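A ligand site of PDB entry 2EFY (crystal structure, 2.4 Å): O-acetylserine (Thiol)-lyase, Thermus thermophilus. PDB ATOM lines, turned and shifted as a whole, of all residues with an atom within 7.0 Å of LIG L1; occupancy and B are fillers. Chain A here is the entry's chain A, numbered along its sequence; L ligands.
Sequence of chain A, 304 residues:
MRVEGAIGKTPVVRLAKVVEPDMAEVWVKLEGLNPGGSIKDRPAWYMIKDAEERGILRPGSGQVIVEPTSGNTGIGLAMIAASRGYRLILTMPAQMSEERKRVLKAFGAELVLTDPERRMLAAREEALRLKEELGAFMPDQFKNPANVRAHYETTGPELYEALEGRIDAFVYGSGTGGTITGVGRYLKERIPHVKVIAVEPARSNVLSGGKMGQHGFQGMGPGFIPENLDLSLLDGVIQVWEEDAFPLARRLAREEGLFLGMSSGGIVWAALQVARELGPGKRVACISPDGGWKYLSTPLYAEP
N of Gly 177 is in hydrogen-bond range of O5 of LG2 L2.
OG1 of Thr 73 is in hydrogen-bond range of O2 of LIG L1.
O5 of LG2 L2 is in hydrogen-bond range of N of Gly 175 (2.8 Å).
The backbone NH of Thr 176 lies within hydrogen-bond range of an oxygen (O3) of LG2 L2.
OG1 of Thr 69 is in hydrogen-bond range of O1 of LIG L1 (2.5 Å).
NZ of Lys 40 is covalently linked to C5 of LG2 L2, 1.3 Å away.
The side-chain hydroxyl of Thr 176 is in hydrogen-bond range of an oxygen (O3) of LG2 L2, 2.6 Å away.
The backbone NH of Thr 73 is in hydrogen-bond range of an oxygen (O2) of LIG L1, at 3.1 Å.
ND2 of Asn 72 lies within hydrogen-bond range of O1 of LG2 L2 (2.6 Å).
N of Asn 72 is in hydrogen-bond range of O2 of LIG L1 (3.2 Å).
The side-chain amino group (NZ) of Lys 40 is in salt-bridge range of an oxygen (O2) of LIG L1, 3.7 Å away.
An oxygen (O1) of LIG L1 is in hydrogen-bond range of the side-chain amide nitrogen (NE2) of Gln 141 (2.9 Å).
Merely in contact with LIG L1: Gly 219 (3.3 Å), Gly 175 (3.3 Å), Pro 222 (3.4 Å), Gly 71 (3.5 Å) and Met 220 (3.8 Å).
Hydrophobic or aromatic side chains within 4 Å of LIG L1: Pro 222.
Ten residues have an atom within 4 Å of LIG L1: Lys 40, Thr 69, Gly 71, Asn 72, Thr 73, Gln 141, Gly 175, Gly 219, Met 220 and Pro 222.
The side-chain hydroxyl (OG1) of Thr 69 sits at hydrogen-bond distance from the backbone NH (N) of Gly 71 (3.2 Å).
The backbone carbonyl oxygen (O) of Met 220 lies close to a ring nitrogen (NE2) of His 215, at 3.2 Å.
The side-chain hydroxyl (OG1) of Thr 73 is in hydrogen-bond range of the side-chain amide oxygen (OE1) of Gln 141, 2.6 Å away.
N of Gln 141 is in hydrogen-bond range of OE2 of Glu 67.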
ATOM      1  N   LYS A  40       4.775  25.704  27.301  1.00  0.00           N
ATOM      2  CA  LYS A  40       5.971  25.508  28.121  1.00  0.00           C
ATOM      3  C   LYS A  40       6.816  26.764  28.354  1.00  0.00           C
ATOM      4  O   LYS A  40       7.673  26.780  29.239  1.00  0.00           O
ATOM      5  CB  LYS A  40       6.839  24.389  27.539  1.00  0.00           C
ATOM      6  CG  LYS A  40       6.252  22.994  27.676  1.00  0.00           C
ATOM      7  CD  LYS A  40       5.903  22.676  29.131  1.00  0.00           C
ATOM      8  CE  LYS A  40       5.732  21.166  29.345  1.00  0.00           C
ATOM      9  NZ  LYS A  40       4.858  20.589  28.301  1.00  0.00           N
ATOM     10  N   GLU A  67      18.445  19.424  31.459  1.00  0.00           N
ATOM     11  CA  GLU A  67      17.125  18.850  31.678  1.00  0.00           C
ATOM     12  C   GLU A  67      16.840  17.757  30.656  1.00  0.00           C
ATOM     13  O   GLU A  67      17.151  17.892  29.464  1.00  0.00           O
ATOM     14  CB  GLU A  67      16.043  19.930  31.545  1.00  0.00           C
ATOM     15  CG  GLU A  67      14.600  19.424  31.748  1.00  0.00           C
ATOM     16  CD  GLU A  67      14.209  19.311  33.216  1.00  0.00           C
ATOM     17  OE1 GLU A  67      15.059  19.603  34.098  1.00  0.00           O
ATOM     18  OE2 GLU A  67      13.049  18.935  33.502  1.00  0.00           O
ATOM     19  N   PRO A  68      16.268  16.637  31.118  1.00  0.00           N
ATOM     20  CA  PRO A  68      15.953  15.541  30.196  1.00  0.00           C
ATOM     21  C   PRO A  68      14.549  15.790  29.638  1.00  0.00           C
ATOM     22  O   PRO A  68      13.549  15.650  30.343  1.00  0.00           O
ATOM     23  CB  PRO A  68      16.005  14.314  31.105  1.00  0.00           C
ATOM     24  CG  PRO A  68      15.482  14.844  32.406  1.00  0.00           C
ATOM     25  CD  PRO A  68      16.156  16.204  32.517  1.00  0.00           C
ATOM     26  N   THR A  69      14.479  16.204  28.375  1.00  0.00           N
ATOM     27  CA  THR A  69      13.185  16.471  27.739  1.00  0.00           C
ATOM     28  C   THR A  69      13.186  16.358  26.217  1.00  0.00           C
ATOM     29  O   THR A  69      14.076  16.874  25.548  1.00  0.00           O
ATOM     30  CB  THR A  69      12.658  17.866  28.075  1.00  0.00           C
ATOM     31  OG1 THR A  69      11.486  18.123  27.277  1.00  0.00           O
ATOM     32  CG2 THR A  69      13.710  18.935  27.784  1.00  0.00           C
ATOM     33  N   SER A  70      12.177  15.671  25.692  1.00  0.00           N
ATOM     34  CA  SER A  70      12.031  15.474  24.254  1.00  0.00           C
ATOM     35  C   SER A  70      10.811  16.212  23.701  1.00  0.00           C
ATOM     36  O   SER A  70      10.287  15.847  22.637  1.00  0.00           O
ATOM     37  CB  SER A  70      11.896  13.970  23.956  1.00  0.00           C
ATOM     38  OG  SER A  70      10.767  13.418  24.620  1.00  0.00           O
ATOM     39  N   GLY A  71      10.353  17.247  24.410  1.00  0.00           N
ATOM     40  CA  GLY A  71       9.195  18.005  23.965  1.00  0.00           C
ATOM     41  C   GLY A  71       9.316  19.516  24.025  1.00  0.00           C
ATOM     42  O   GLY A  71      10.404  20.075  23.892  1.00  0.00           O
ATOM     43  N   ASN A  72       8.189  20.186  24.232  1.00  0.00           N
ATOM     44  CA  ASN A  72       8.145  21.641  24.310  1.00  0.00           C
ATOM     45  C   ASN A  72       8.998  22.254  25.418  1.00  0.00           C
ATOM     46  O   ASN A  72       9.462  23.384  25.273  1.00  0.00           O
ATOM     47  CB  ASN A  72       6.695  22.129  24.457  1.00  0.00           C
ATOM     48  CG  ASN A  72       5.874  21.878  23.213  1.00  0.00           C
ATOM     49  OD1 ASN A  72       6.258  22.283  22.121  1.00  0.00           O
ATOM     50  ND2 ASN A  72       4.737  21.209  23.374  1.00  0.00           N
ATOM     51  N   THR A  73       9.203  21.533  26.517  1.00  0.00           N
ATOM     52  CA  THR A  73      10.023  22.091  27.584  1.00  0.00           C
ATOM     53  C   THR A  73      11.442  22.388  27.096  1.00  0.00           C
ATOM     54  O   THR A  73      11.999  23.441  27.415  1.00  0.00           O
ATOM     55  CB  THR A  73      10.090  21.154  28.819  1.00  0.00           C
ATOM     56  OG1 THR A  73       8.772  20.991  29.356  1.00  0.00           O
ATOM     57  CG2 THR A  73      10.986  21.749  29.898  1.00  0.00           C
ATOM     58  N   GLY A  74      12.004  21.477  26.307  1.00  0.00           N
ATOM     59  CA  GLY A  74      13.338  21.697  25.772  1.00  0.00           C
ATOM     60  C   GLY A  74      13.381  22.974  24.969  1.00  0.00           C
ATOM     61  O   GLY A  74      14.351  23.731  25.034  1.00  0.00           O
ATOM     62  N   ILE A  75      12.315  23.225  24.208  1.00  0.00           N
ATOM     63  CA  ILE A  75      12.235  24.422  23.380  1.00  0.00           C
ATOM     64  C   ILE A  75      12.091  25.659  24.243  1.00  0.00           C
ATOM     65  O   ILE A  75      12.784  26.645  24.032  1.00  0.00           O
ATOM     66  CB  ILE A  75      11.034  24.326  22.406  1.00  0.00           C
ATOM     67  CG1 ILE A  75      11.225  23.126  21.473  1.00  0.00           C
ATOM     68  CG2 ILE A  75      10.911  25.621  21.586  1.00  0.00           C
ATOM     69  CD1 ILE A  75      10.015  22.797  20.634  1.00  0.00           C
ATOM     70  N   GLN A 141      11.205  19.501  35.720  1.00  0.00           N
ATOM     71  CA  GLN A 141       9.840  19.905  35.414  1.00  0.00           C
ATOM     72  C   GLN A 141       8.680  19.181  36.084  1.00  0.00           C
ATOM     73  O   GLN A 141       7.597  19.753  36.213  1.00  0.00           O
ATOM     74  CB  GLN A 141       9.620  19.877  33.891  1.00  0.00           C
ATOM     75  CG  GLN A 141       9.512  18.472  33.307  1.00  0.00           C
ATOM     76  CD  GLN A 141       9.327  18.493  31.794  1.00  0.00           C
ATOM     77  OE1 GLN A 141       8.499  19.226  31.278  1.00  0.00           O
ATOM     78  NE2 GLN A 141      10.099  17.673  31.100  1.00  0.00           N
ATOM     79  N   PHE A 142       8.877  17.920  36.485  1.00  0.00           N
ATOM     80  CA  PHE A 142       7.794  17.166  37.120  1.00  0.00           C
ATOM     81  C   PHE A 142       7.676  17.376  38.635  1.00  0.00           C
ATOM     82  O   PHE A 142       6.609  17.104  39.213  1.00  0.00           O
ATOM     83  CB  PHE A 142       7.937  15.669  36.844  1.00  0.00           C
ATOM     84  CG  PHE A 142       7.770  15.287  35.401  1.00  0.00           C
ATOM     85  CD1 PHE A 142       8.869  15.188  34.544  1.00  0.00           C
ATOM     86  CD2 PHE A 142       6.499  14.981  34.889  1.00  0.00           C
ATOM     87  CE1 PHE A 142       8.712  14.804  33.203  1.00  0.00           C
ATOM     88  CE2 PHE A 142       6.332  14.596  33.558  1.00  0.00           C
ATOM     89  CZ  PHE A 142       7.442  14.505  32.704  1.00  0.00           C
ATOM     90  N   SER A 174      -3.348  16.613  31.434  1.00  0.00           N
ATOM     91  CA  SER A 174      -2.163  16.721  32.271  1.00  0.00           C
ATOM     92  C   SER A 174      -0.890  16.032  31.794  1.00  0.00           C
ATOM     93  O   SER A 174      -0.911  14.895  31.323  1.00  0.00           O
ATOM     94  CB  SER A 174      -2.494  16.252  33.685  1.00  0.00           C
ATOM     95  OG  SER A 174      -1.439  16.579  34.578  1.00  0.00           O
ATOM     96  N   GLY A 175       0.221  16.751  31.928  1.00  0.00           N
ATOM     97  CA  GLY A 175       1.526  16.230  31.556  1.00  0.00           C
ATOM     98  C   GLY A 175       2.408  16.284  32.797  1.00  0.00           C
ATOM     99  O   GLY A 175       2.484  15.327  33.560  1.00  0.00           O
ATOM    100  N   THR A 176       3.074  17.421  33.015  1.00  0.00           N
ATOM    101  CA  THR A 176       3.898  17.564  34.207  1.00  0.00           C
ATOM    102  C   THR A 176       2.956  17.771  35.393  1.00  0.00           C
ATOM    103  O   THR A 176       3.349  17.584  36.538  1.00  0.00           O
ATOM    104  CB  THR A 176       4.855  18.779  34.144  1.00  0.00           C
ATOM    105  OG1 THR A 176       4.092  19.977  34.069  1.00  0.00           O
ATOM    106  CG2 THR A 176       5.783  18.673  32.935  1.00  0.00           C
ATOM    107  N   GLY A 177       1.717  18.157  35.103  1.00  0.00           N
ATOM    108  CA  GLY A 177       0.742  18.404  36.157  1.00  0.00           C
ATOM    109  C   GLY A 177       0.698  19.864  36.571  1.00  0.00           C
ATOM    110  O   GLY A 177      -0.182  20.299  37.319  1.00  0.00           O
ATOM    111  N   HIS A 215       0.972   5.811  23.479  1.00  0.00           N
ATOM    112  CA  HIS A 215      -0.178   6.592  23.014  1.00  0.00           C
ATOM    113  C   HIS A 215       0.374   7.758  22.211  1.00  0.00           C
ATOM    114  O   HIS A 215       1.505   8.189  22.462  1.00  0.00           O
ATOM    115  CB  HIS A 215      -0.992   7.102  24.207  1.00  0.00           C
ATOM    116  CG  HIS A 215      -0.291   8.134  25.028  1.00  0.00           C
ATOM    117  ND1 HIS A 215      -0.151   9.441  24.623  1.00  0.00           N
ATOM    118  CD2 HIS A 215       0.334   8.056  26.232  1.00  0.00           C
ATOM    119  CE1 HIS A 215       0.521  10.124  25.534  1.00  0.00           C
ATOM    120  NE2 HIS A 215       0.824   9.302  26.517  1.00  0.00           N
ATOM    121  N   PHE A 217      -0.639  11.037  22.049  1.00  0.00           N
ATOM    122  CA  PHE A 217      -0.858  12.401  22.515  1.00  0.00           C
ATOM    123  C   PHE A 217       0.430  13.008  23.072  1.00  0.00           C
ATOM    124  O   PHE A 217       0.623  13.064  24.287  1.00  0.00           O
ATOM    125  CB  PHE A 217      -1.952  12.428  23.603  1.00  0.00           C
ATOM    126  CG  PHE A 217      -3.296  11.984  23.111  1.00  0.00           C
ATOM    127  CD1 PHE A 217      -3.725  10.680  23.309  1.00  0.00           C
ATOM    128  CD2 PHE A 217      -4.113  12.869  22.411  1.00  0.00           C
ATOM    129  CE1 PHE A 217      -4.959  10.254  22.810  1.00  0.00           C
ATOM    130  CE2 PHE A 217      -5.342  12.451  21.907  1.00  0.00           C
ATOM    131  CZ  PHE A 217      -5.765  11.147  22.113  1.00  0.00           C
ATOM    132  N   GLN A 218       1.306  13.466  22.187  1.00  0.00           N
ATOM    133  CA  GLN A 218       2.577  14.034  22.631  1.00  0.00           C
ATOM    134  C   GLN A 218       2.432  15.236  23.549  1.00  0.00           C
ATOM    135  O   GLN A 218       1.673  16.162  23.271  1.00  0.00           O
ATOM    136  CB  GLN A 218       3.435  14.429  21.424  1.00  0.00           C
ATOM    137  CG  GLN A 218       3.622  13.293  20.414  1.00  0.00           C
ATOM    138  CD  GLN A 218       4.496  13.679  19.233  1.00  0.00           C
ATOM    139  OE1 GLN A 218       4.389  13.095  18.153  1.00  0.00           O
ATOM    140  NE2 GLN A 218       5.373  14.654  19.444  1.00  0.00           N
ATOM    141  N   GLY A 219       3.146  15.197  24.668  1.00  0.00           N
ATOM    142  CA  GLY A 219       3.097  16.287  25.610  1.00  0.00           C
ATOM    143  C   GLY A 219       2.335  15.960  26.883  1.00  0.00           C
ATOM    144  O   GLY A 219       2.623  16.539  27.925  1.00  0.00           O
ATOM    145  N   MET A 220       1.394  15.035  26.807  1.00  0.00           N
ATOM    146  CA  MET A 220       0.614  14.672  27.995  1.00  0.00           C
ATOM    147  C   MET A 220       0.637  13.156  28.256  1.00  0.00           C
ATOM    148  O   MET A 220       1.151  12.373  27.453  1.00  0.00           O
ATOM    149  CB  MET A 220      -0.832  15.153  27.830  1.00  0.00           C
ATOM    150  CG  MET A 220      -1.527  14.548  26.610  1.00  0.00           C
ATOM    151  SD  MET A 220      -3.292  14.932  26.471  1.00  0.00           S
ATOM    152  CE  MET A 220      -3.994  13.713  27.571  1.00  0.00           C
ATOM    153  N   GLY A 221       0.056  12.740  29.388  1.00  0.00           N
ATOM    154  CA  GLY A 221       0.015  11.330  29.718  1.00  0.00           C
ATOM    155  C   GLY A 221       1.413  10.748  29.883  1.00  0.00           C
ATOM    156  O   GLY A 221       1.816   9.875  29.097  1.00  0.00           O
ATOM    157  N   PRO A 222       2.175  11.204  30.888  1.00  0.00           N
ATOM    158  CA  PRO A 222       3.537  10.783  31.209  1.00  0.00           C
ATOM    159  C   PRO A 222       3.666   9.309  31.594  1.00  0.00           C
ATOM    160  O   PRO A 222       4.763   8.733  31.520  1.00  0.00           O
ATOM    161  CB  PRO A 222       3.926  11.712  32.358  1.00  0.00           C
ATOM    162  CG  PRO A 222       2.639  11.843  33.107  1.00  0.00           C
ATOM    163  CD  PRO A 222       1.633  12.059  31.976  1.00  0.00           C
ATOM    164  N   GLY A 223       2.573   8.709  32.023  1.00  0.00           N
ATOM    165  CA  GLY A 223       2.615   7.311  32.399  1.00  0.00           C
ATOM    166  C   GLY A 223       2.781   7.106  33.890  1.00  0.00           C
ATOM    167  O   GLY A 223       3.055   5.993  34.338  1.00  0.00           O
ATOM    168  N   PHE A 224       2.628   8.188  34.654  1.00  0.00           N
ATOM    169  CA  PHE A 224       2.736   8.133  36.113  1.00  0.00           C
ATOM    170  C   PHE A 224       2.196   9.432  36.709  1.00  0.00           C
ATOM    171  O   PHE A 224       1.915  10.379  35.978  1.00  0.00           O
ATOM    172  CB  PHE A 224       4.200   7.933  36.545  1.00  0.00           C
ATOM    173  CG  PHE A 224       5.080   9.133  36.319  1.00  0.00           C
ATOM    174  CD1 PHE A 224       5.212  10.104  37.301  1.00  0.00           C
ATOM    175  CD2 PHE A 224       5.774   9.281  35.117  1.00  0.00           C
ATOM    176  CE1 PHE A 224       6.043  11.208  37.103  1.00  0.00           C
ATOM    177  CE2 PHE A 224       6.598  10.385  34.912  1.00  0.00           C
ATOM    178  CZ  PHE A 224       6.737  11.356  35.901  1.00  0.00           C
HETATM  179  C1  LIG L   1       8.190  17.952  28.069  1.00  0.00           C
HETATM  180  O1  LIG L   1       9.261  17.540  28.284  1.00  0.00           O
HETATM  181  O2  LIG L   1       7.835  18.809  27.139  1.00  0.00           O
HETATM  182  C2  LIG L   1       7.004  17.478  28.948  1.00  0.00           C
HETATM  183  C3  LIG L   1       6.603  16.063  28.510  1.00  0.00           C
HETATM  184  C4  LIG L   1       5.481  15.684  29.304  1.00  0.00           C
HETATM  185  C5  LIG L   1       3.728  14.262  30.091  1.00  0.00           C
HETATM  186  C6  LIG L   1       4.887  14.510  29.196  1.00  0.00           C
HETATM  187  O3  LIG L   1       5.245  13.652  28.387  1.00  0.00           O
HETATM  188  N1  LG2 L   2       0.612  19.003  25.817  1.00  0.00           N
HETATM  189  C1  LG2 L   2       1.790  19.483  25.339  1.00  0.00           C
HETATM  190  C2  LG2 L   2       2.002  19.472  23.772  1.00  0.00           C
HETATM  191  C3  LG2 L   2       2.766  19.957  26.220  1.00  0.00           C
HETATM  192  O1  LG2 L   2       3.940  20.415  25.744  1.00  0.00           O
HETATM  193  C4  LG2 L   2       2.520  19.935  27.594  1.00  0.00           C
HETATM  194  C5  LG2 L   2       3.553  20.460  28.562  1.00  0.00           C
HETATM  195  C6  LG2 L   2       1.282  19.433  28.060  1.00  0.00           C
HETATM  196  C7  LG2 L   2       0.359  18.991  27.156  1.00  0.00           C
HETATM  197  C8  LG2 L   2       0.858  19.324  29.546  1.00  0.00           C
HETATM  198  O2  LG2 L   2       0.877  20.469  30.453  1.00  0.00           O
HETATM  199  P1  LG2 L   2       1.549  20.226  31.909  1.00  0.00           P
HETATM  200  O3  LG2 L   2       2.961  19.815  31.763  1.00  0.00           O
HETATM  201  O4  LG2 L   2       1.539  21.698  32.501  1.00  0.00           O
HETATM  202  O5  LG2 L   2       0.657  19.365  32.686  1.00  0.00           O
